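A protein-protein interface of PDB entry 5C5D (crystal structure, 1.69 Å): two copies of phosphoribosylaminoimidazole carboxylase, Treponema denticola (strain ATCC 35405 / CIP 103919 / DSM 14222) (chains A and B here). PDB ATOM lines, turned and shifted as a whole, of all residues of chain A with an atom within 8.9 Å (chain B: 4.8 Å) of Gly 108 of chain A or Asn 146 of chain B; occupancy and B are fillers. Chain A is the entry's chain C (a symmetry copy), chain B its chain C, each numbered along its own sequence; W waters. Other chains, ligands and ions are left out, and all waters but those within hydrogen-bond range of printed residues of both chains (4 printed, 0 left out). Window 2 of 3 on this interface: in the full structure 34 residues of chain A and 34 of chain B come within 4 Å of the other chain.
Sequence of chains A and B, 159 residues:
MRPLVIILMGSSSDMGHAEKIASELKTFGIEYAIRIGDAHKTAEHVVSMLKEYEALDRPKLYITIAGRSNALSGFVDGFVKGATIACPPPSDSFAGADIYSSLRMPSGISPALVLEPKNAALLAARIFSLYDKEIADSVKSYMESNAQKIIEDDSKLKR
The backbone NH (N) of Ser 110 of chain A sits at hydrogen-bond distance from the side-chain carboxylate (OD2) of Asp 77 of chain A (2.8 Å).
Water W4 lies within hydrogen-bond range of the backbone carbonyl oxygen of Gly 108 of chain A (2.8 Å) and the side-chain amide nitrogen of Asn 146 of chain B (3.0 Å).
Water W2 lies within hydrogen-bond range of OG of Ser 107 of chain A (2.8 Å), OH of Tyr 142 of chain B (3.0 Å), ND2 of Asn 146 of chain B (3.2 Å) and N of Gly 108 of chain A (3.3 Å).
Water W3 lies within hydrogen-bond range of the backbone carbonyl oxygen of Ile 109 of chain A (2.9 Å) and the side-chain amide nitrogen of Asn 119 of chain B (3.0 Å).
Water W1 lies within hydrogen-bond range of OH of Tyr 142 of chain B (2.9 Å), OD1 of Asn 119 of chain B (3.0 Å) and N of Gly 108 of chain A (3.1 Å).
Among the printed residues, merely in contact across the chains: Asp 77 of chain A with Met 143 of chain B (3.6 Å), Ser 107 of chain A with Asn 119 of chain B (3.7 Å), Gly 108 of chain A with Leu 122 of chain B (3.6 Å), Gly 108 of chain A with Met 143 of chain B (3.6 Å), Gly 108 of chain A with Asn 146 of chain B (3.8 Å), Ser 110 of chain A with Asn 119 of chain B (3.5 Å) and Ser 110 of chain A with Leu 122 of chain B (3.6 Å).
No position is printed for both chains.
Of the 10 pairs that touch across the chains among the printed residues, none has its exchanged pair printed and touching as well.
Of the 11 printed residues of chain B, 4 touch a printed residue of chain A.
Hydrophobic or aromatic side chains of chain B within 4 Å of the printed part of chain A: Leu 122 and Met 143.
The backbone NH of Gly 108 of chain A is in hydrogen-bond range of the side-chain amide oxygen of Asn 119 of chain B (2.8 Å).
The backbone carbonyl oxygen (O) of Pro 106 of chain A sits at hydrogen-bond distance from the side-chain amide nitrogen (ND2) of Asn 119 of chain B, at 3.0 Å.
The backbone carbonyl oxygen (O) of Ile 109 of chain A lies within hydrogen-bond range of the side-chain amide nitrogen (ND2) of Asn 119 of chain B.
Val 80 of chain A touches none of the printed residues of chain B.
Printed residues of chain B within 4 Å of Gly 108 of chain A: Asn 119, Leu 122, Met 143 and Asn 146.
Printed residues of chain A within 4 Å of Asn 119 of chain B: Pro 106 (3.0 Å), Ser 107 (3.7 Å), Gly 108 (2.8 Å), Ile 109 (3.0 Å) and Ser 110 (3.5 Å).
Of the printed residues of chain A, Met 143 of chain B touches Asp 77 and Gly 108.
Glu 144 of chain B touches none of the printed residues of chain A.
No residue of chain A comes within 4 Å of Ser 145 of chain B.
Of chain A, only Gly 108 (3.8 Å) comes within 4 Å of Asn 146 of chain B.
No residue of chain A comes within 4 Å of Ala 147 of chain B.
The nearest residue of chain A that does not touch Asn 146 of chain B is Ser 107 of chain A (4.6 Å).
The nearest printed residue of chain B that does not touch Ser 107 of chain A is Asn 146 of chain B (4.6 Å).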
ATOM      1  N   GLY A  74      13.540  32.821  14.285  1.00  0.00           N
ATOM      2  CA  GLY A  74      12.824  31.567  14.149  1.00  0.00           C
ATOM      3  C   GLY A  74      11.829  31.578  13.026  1.00  0.00           C
ATOM      4  O   GLY A  74      11.615  30.559  12.390  1.00  0.00           O
ATOM      5  N   ASP A  77      13.885  31.266   9.883  1.00  0.00           N
ATOM      6  CA  ASP A  77      14.444  29.936   9.846  1.00  0.00           C
ATOM      7  C   ASP A  77      13.401  28.844   9.516  1.00  0.00           C
ATOM      8  O   ASP A  77      13.709  27.859   8.845  1.00  0.00           O
ATOM      9  CB  ASP A  77      15.129  29.625  11.171  1.00  0.00           C
ATOM     10  CG  ASP A  77      15.999  28.408  11.085  1.00  0.00           C
ATOM     11  OD1 ASP A  77      17.151  28.530  10.592  1.00  0.00           O
ATOM     12  OD2 ASP A  77      15.538  27.309  11.444  1.00  0.00           O
ATOM     13  N   GLY A  78      12.166  29.015   9.977  1.00  0.00           N
ATOM     14  CA  GLY A  78      11.148  28.031   9.654  1.00  0.00           C
ATOM     15  C   GLY A  78      10.592  28.165   8.250  1.00  0.00           C
ATOM     16  O   GLY A  78       9.908  27.261   7.776  1.00  0.00           O
ATOM     17  N   PHE A  79      10.931  29.258   7.563  1.00  0.00           N
ATOM     18  CA  PHE A  79      10.429  29.487   6.199  1.00  0.00           C
ATOM     19  C   PHE A  79      11.438  29.077   5.117  1.00  0.00           C
ATOM     20  O   PHE A  79      11.077  28.413   4.139  1.00  0.00           O
ATOM     21  CB  PHE A  79      10.041  30.958   6.014  1.00  0.00           C
ATOM     22  CG  PHE A  79       9.368  31.213   4.700  1.00  0.00           C
ATOM     23  CD1 PHE A  79       7.997  31.123   4.587  1.00  0.00           C
ATOM     24  CD2 PHE A  79      10.118  31.469   3.570  1.00  0.00           C
ATOM     25  CE1 PHE A  79       7.381  31.327   3.369  1.00  0.00           C
ATOM     26  CE2 PHE A  79       9.507  31.667   2.346  1.00  0.00           C
ATOM     27  CZ  PHE A  79       8.143  31.598   2.248  1.00  0.00           C
ATOM     28  N   VAL A  80      12.694  29.455   5.288  1.00  0.00           N
ATOM     29  CA  VAL A  80      13.683  29.299   4.218  1.00  0.00           C
ATOM     30  C   VAL A  80      14.267  27.911   4.247  1.00  0.00           C
ATOM     31  O   VAL A  80      14.170  27.195   5.232  1.00  0.00           O
ATOM     32  CB  VAL A  80      14.804  30.347   4.308  1.00  0.00           C
ATOM     33  CG1 VAL A  80      14.203  31.754   4.268  1.00  0.00           C
ATOM     34  CG2 VAL A  80      15.667  30.139   5.571  1.00  0.00           C
ATOM     35  N   MET A 105      14.963  27.658  20.990  1.00  0.00           N
ATOM     36  CA  MET A 105      14.172  27.252  19.850  1.00  0.00           C
ATOM     37  C   MET A 105      13.524  25.875  20.085  1.00  0.00           C
ATOM     38  O   MET A 105      14.046  25.045  20.818  1.00  0.00           O
ATOM     39  CB  MET A 105      15.083  27.227  18.601  1.00  0.00           C
ATOM     40  CG  MET A 105      15.672  28.544  18.284  1.00  0.00           C
ATOM     41  SD  MET A 105      14.376  29.753  17.791  1.00  0.00           S
ATOM     42  CE  MET A 105      14.019  30.691  19.360  1.00  0.00           C
ATOM     43  N   PRO A 106      12.377  25.638  19.450  1.00  0.00           N
ATOM     44  CA  PRO A 106      11.775  24.298  19.410  1.00  0.00           C
ATOM     45  C   PRO A 106      12.649  23.360  18.571  1.00  0.00           C
ATOM     46  O   PRO A 106      13.464  23.810  17.805  1.00  0.00           O
ATOM     47  CB  PRO A 106      10.408  24.548  18.778  1.00  0.00           C
ATOM     48  CG  PRO A 106      10.584  25.704  17.909  1.00  0.00           C
ATOM     49  CD  PRO A 106      11.647  26.591  18.611  1.00  0.00           C
ATOM     50  N   SER A 107      12.519  22.058  18.755  1.00  0.00           N
ATOM     51  CA  SER A 107      13.167  21.128  17.849  1.00  0.00           C
ATOM     52  C   SER A 107      12.646  21.416  16.442  1.00  0.00           C
ATOM     53  O   SER A 107      11.447  21.591  16.257  1.00  0.00           O
ATOM     54  CB  SER A 107      12.862  19.687  18.247  1.00  0.00           C
ATOM     55  OG  SER A 107      13.655  18.792  17.490  1.00  0.00           O
ATOM     56  N   GLY A 108      13.529  21.470  15.444  1.00  0.00           N
ATOM     57  CA  GLY A 108      13.091  21.734  14.076  1.00  0.00           C
ATOM     58  C   GLY A 108      13.302  23.157  13.580  1.00  0.00           C
ATOM     59  O   GLY A 108      13.049  23.469  12.427  1.00  0.00           O
ATOM     60  N   ILE A 109      13.768  24.043  14.466  1.00  0.00           N
ATOM     61  CA  ILE A 109      14.084  25.425  14.131  1.00  0.00           C
ATOM     62  C   ILE A 109      15.529  25.627  14.575  1.00  0.00           C
ATOM     63  O   ILE A 109      15.825  25.531  15.766  1.00  0.00           O
ATOM     64  CB  ILE A 109      13.142  26.426  14.809  1.00  0.00           C
ATOM     65  CG1 ILE A 109      11.718  26.232  14.261  1.00  0.00           C
ATOM     66  CG2 ILE A 109      13.639  27.858  14.574  1.00  0.00           C
ATOM     67  CD1 ILE A 109      11.559  26.596  12.790  1.00  0.00           C
ATOM     68  N   SER A 110      16.435  25.877  13.629  1.00  0.00           N
ATOM     69  CA  SER A 110      17.846  25.723  13.915  1.00  0.00           C
ATOM     70  C   SER A 110      18.750  26.868  13.514  1.00  0.00           C
ATOM     71  O   SER A 110      19.818  26.610  12.946  1.00  0.00           O
ATOM     72  CB  SER A 110      18.361  24.449  13.221  1.00  0.00           C
ATOM     73  OG  SER A 110      18.292  24.619  11.816  1.00  0.00           O
ATOM     74  N   PRO A 111      18.391  28.123  13.830  1.00  0.00           N
ATOM     75  CA  PRO A 111      19.326  29.207  13.515  1.00  0.00           C
ATOM     76  C   PRO A 111      20.610  29.088  14.331  1.00  0.00           C
ATOM     77  O   PRO A 111      20.584  28.701  15.498  1.00  0.00           O
ATOM     78  CB  PRO A 111      18.545  30.455  13.890  1.00  0.00           C
ATOM     79  CG  PRO A 111      17.566  29.994  14.877  1.00  0.00           C
ATOM     80  CD  PRO A 111      17.190  28.644  14.505  1.00  0.00           C
ATOM     81  N   ASN B 119      18.720  19.979  16.617  1.00  0.00           N
ATOM     82  CA  ASN B 119      18.878  21.220  15.857  1.00  0.00           C
ATOM     83  C   ASN B 119      20.327  21.382  15.428  1.00  0.00           C
ATOM     84  O   ASN B 119      20.570  21.977  14.386  1.00  0.00           O
ATOM     85  CB  ASN B 119      18.418  22.444  16.652  1.00  0.00           C
ATOM     86  CG  ASN B 119      16.918  22.570  16.681  1.00  0.00           C
ATOM     87  OD1 ASN B 119      16.228  21.983  15.844  1.00  0.00           O
ATOM     88  ND2 ASN B 119      16.387  23.300  17.670  1.00  0.00           N
ATOM     89  N   LEU B 122      20.316  19.394  12.303  1.00  0.00           N
ATOM     90  CA  LEU B 122      19.576  20.098  11.249  1.00  0.00           C
ATOM     91  C   LEU B 122      20.376  21.301  10.725  1.00  0.00           C
ATOM     92  O   LEU B 122      20.433  21.507   9.505  1.00  0.00           O
ATOM     93  CB  LEU B 122      18.214  20.563  11.761  1.00  0.00           C
ATOM     94  CG  LEU B 122      17.328  21.334  10.780  1.00  0.00           C
ATOM     95  CD1 LEU B 122      16.995  20.502   9.554  1.00  0.00           C
ATOM     96  CD2 LEU B 122      16.043  21.772  11.502  1.00  0.00           C
ATOM     97  N   TYR B 142      12.076  16.570   5.991  1.00  0.00           N
ATOM     98  CA  TYR B 142      12.152  16.599   7.431  1.00  0.00           C
ATOM     99  C   TYR B 142      11.348  17.765   7.966  1.00  0.00           C
ATOM    100  O   TYR B 142      10.528  17.607   8.864  1.00  0.00           O
ATOM    101  CB  TYR B 142      13.616  16.714   7.841  1.00  0.00           C
ATOM    102  CG  TYR B 142      13.962  16.736   9.308  1.00  0.00           C
ATOM    103  CD1 TYR B 142      14.386  15.566   9.947  1.00  0.00           C
ATOM    104  CD2 TYR B 142      13.984  17.918  10.023  1.00  0.00           C
ATOM    105  CE1 TYR B 142      14.768  15.570  11.271  1.00  0.00           C
ATOM    106  CE2 TYR B 142      14.384  17.935  11.380  1.00  0.00           C
ATOM    107  CZ  TYR B 142      14.760  16.756  11.982  1.00  0.00           C
ATOM    108  OH  TYR B 142      15.150  16.730  13.301  1.00  0.00           O
ATOM    109  N   MET B 143      11.589  18.952   7.424  1.00  0.00           N
ATOM    110  CA  MET B 143      10.939  20.130   7.963  1.00  0.00           C
ATOM    111  C   MET B 143       9.444  20.099   7.613  1.00  0.00           C
ATOM    112  O   MET B 143       8.613  20.433   8.458  1.00  0.00           O
ATOM    113  CB  MET B 143      11.644  21.395   7.463  1.00  0.00           C
ATOM    114  CG  MET B 143      12.951  21.597   8.221  1.00  0.00           C
ATOM    115  SD  MET B 143      13.841  23.120   7.889  1.00  0.00           S
ATOM    116  CE  MET B 143      13.026  24.298   8.968  1.00  0.00           C
ATOM    117  N   GLU B 144       9.088  19.657   6.410  1.00  0.00           N
ATOM    118  CA  GLU B 144       7.671  19.509   6.054  1.00  0.00           C
ATOM    119  C   GLU B 144       6.955  18.499   6.946  1.00  0.00           C
ATOM    120  O   GLU B 144       5.798  18.717   7.341  1.00  0.00           O
ATOM    121  CB  GLU B 144       7.509  19.117   4.581  1.00  0.00           C
ATOM    122  CG  GLU B 144       7.763  20.287   3.655  1.00  0.00           C
ATOM    123  CD  GLU B 144       7.615  19.925   2.189  1.00  0.00           C
ATOM    124  OE1 GLU B 144       7.240  18.775   1.894  1.00  0.00           O
ATOM    125  OE2 GLU B 144       7.888  20.794   1.336  1.00  0.00           O
ATOM    126  N   SER B 145       7.646  17.421   7.305  1.00  0.00           N
ATOM    127  CA  SER B 145       7.065  16.408   8.184  1.00  0.00           C
ATOM    128  C   SER B 145       6.802  16.975   9.595  1.00  0.00           C
ATOM    129  O   SER B 145       5.783  16.660  10.228  1.00  0.00           O
ATOM    130  CB  SER B 145       7.984  15.196   8.265  1.00  0.00           C
ATOM    131  OG  SER B 145       7.586  14.365   9.332  1.00  0.00           O
ATOM    132  N   ASN B 146       7.708  17.805  10.074  1.00  0.00           N
ATOM    133  CA  ASN B 146       7.523  18.460  11.374  1.00  0.00           C
ATOM    134  C   ASN B 146       6.307  19.375  11.353  1.00  0.00           C
ATOM    135  O   ASN B 146       5.535  19.404  12.314  1.00  0.00           O
ATOM    136  CB  ASN B 146       8.748  19.266  11.778  1.00  0.00           C
ATOM    137  CG  ASN B 146       9.849  18.410  12.354  1.00  0.00           C
ATOM    138  OD1 ASN B 146       9.638  17.248  12.687  1.00  0.00           O
ATOM    139  ND2 ASN B 146      11.037  18.979  12.471  1.00  0.00           N
ATOM    140  N   ALA B 147       6.117  20.112  10.263  1.00  0.00           N
ATOM    141  CA  ALA B 147       4.978  21.010  10.194  1.00  0.00           C
ATOM    142  C   ALA B 147       3.691  20.198  10.104  1.00  0.00           C
ATOM    143  O   ALA B 147       2.689  20.512  10.747  1.00  0.00           O
ATOM    144  CB  ALA B 147       5.103  21.958   9.018  1.00  0.00           C
ATOM    145  N   GLN B 148       3.711  19.129   9.317  1.00  0.00           N
ATOM    146  CA  GLN B 148       2.516  18.328   9.147  1.00  0.00           C
ATOM    147  C   GLN B 148       2.063  17.638  10.427  1.00  0.00           C
ATOM    148  O   GLN B 148       0.858  17.457  10.624  1.00  0.00           O
ATOM    149  CB  GLN B 148       2.726  17.281   8.054  1.00  0.00           C
ATOM    150  CG  GLN B 148       2.358  17.779   6.662  1.00  0.00           C
ATOM    151  CD  GLN B 148       0.938  18.335   6.582  1.00  0.00           C
ATOM    152  OE1 GLN B 148      -0.037  17.636   6.866  1.00  0.00           O
ATOM    153  NE2 GLN B 148       0.824  19.605   6.211  1.00  0.00           N
ATOM    154  N   LYS B 149       2.999  17.257  11.286  1.00  0.00           N
ATOM    155  CA  LYS B 149       2.635  16.599  12.552  1.00  0.00           C
ATOM    156  C   LYS B 149       1.817  17.562  13.418  1.00  0.00           C
ATOM    157  O   LYS B 149       0.836  17.176  14.053  1.00  0.00           O
ATOM    158  CB  LYS B 149       3.878  16.124  13.313  1.00  0.00           C
ATOM    159  CG  LYS B 149       3.574  15.406  14.630  1.00  0.00           C
ATOM    160  CD  LYS B 149       3.979  16.244  15.848  1.00  0.00           C
ATOM    161  CE  LYS B 149       3.565  15.584  17.160  1.00  0.00           C
ATOM    162  NZ  LYS B 149       3.910  16.421  18.340  1.00  0.00           N
ATOM    163  N   ILE B 150       2.212  18.824  13.418  1.00  0.00           N
ATOM    164  CA  ILE B 150       1.495  19.834  14.222  1.00  0.00           C
ATOM    165  C   ILE B 150       0.083  20.056  13.718  1.00  0.00           C
ATOM    166  O   ILE B 150      -0.903  20.093  14.488  1.00  0.00           O
ATOM    167  CB  ILE B 150       2.287  21.137  14.209  1.00  0.00           C
ATOM    168  CG1 ILE B 150       3.619  20.891  14.909  1.00  0.00           C
ATOM    169  CG2 ILE B 150       1.512  22.272  14.874  1.00  0.00           C
ATOM    170  CD1 ILE B 150       4.708  21.864  14.538  1.00  0.00           C
HETATM  171  O   HOH W   1      15.590  19.451  14.352  1.00  0.00           O
HETATM  172  O   HOH W   2      13.053  18.227  14.773  1.00  0.00           O
HETATM  173  O   HOH W   3      18.076  25.741  17.587  1.00  0.00           O
HETATM  174  O   HOH W   4      11.232  21.674  11.277  1.00  0.00           O
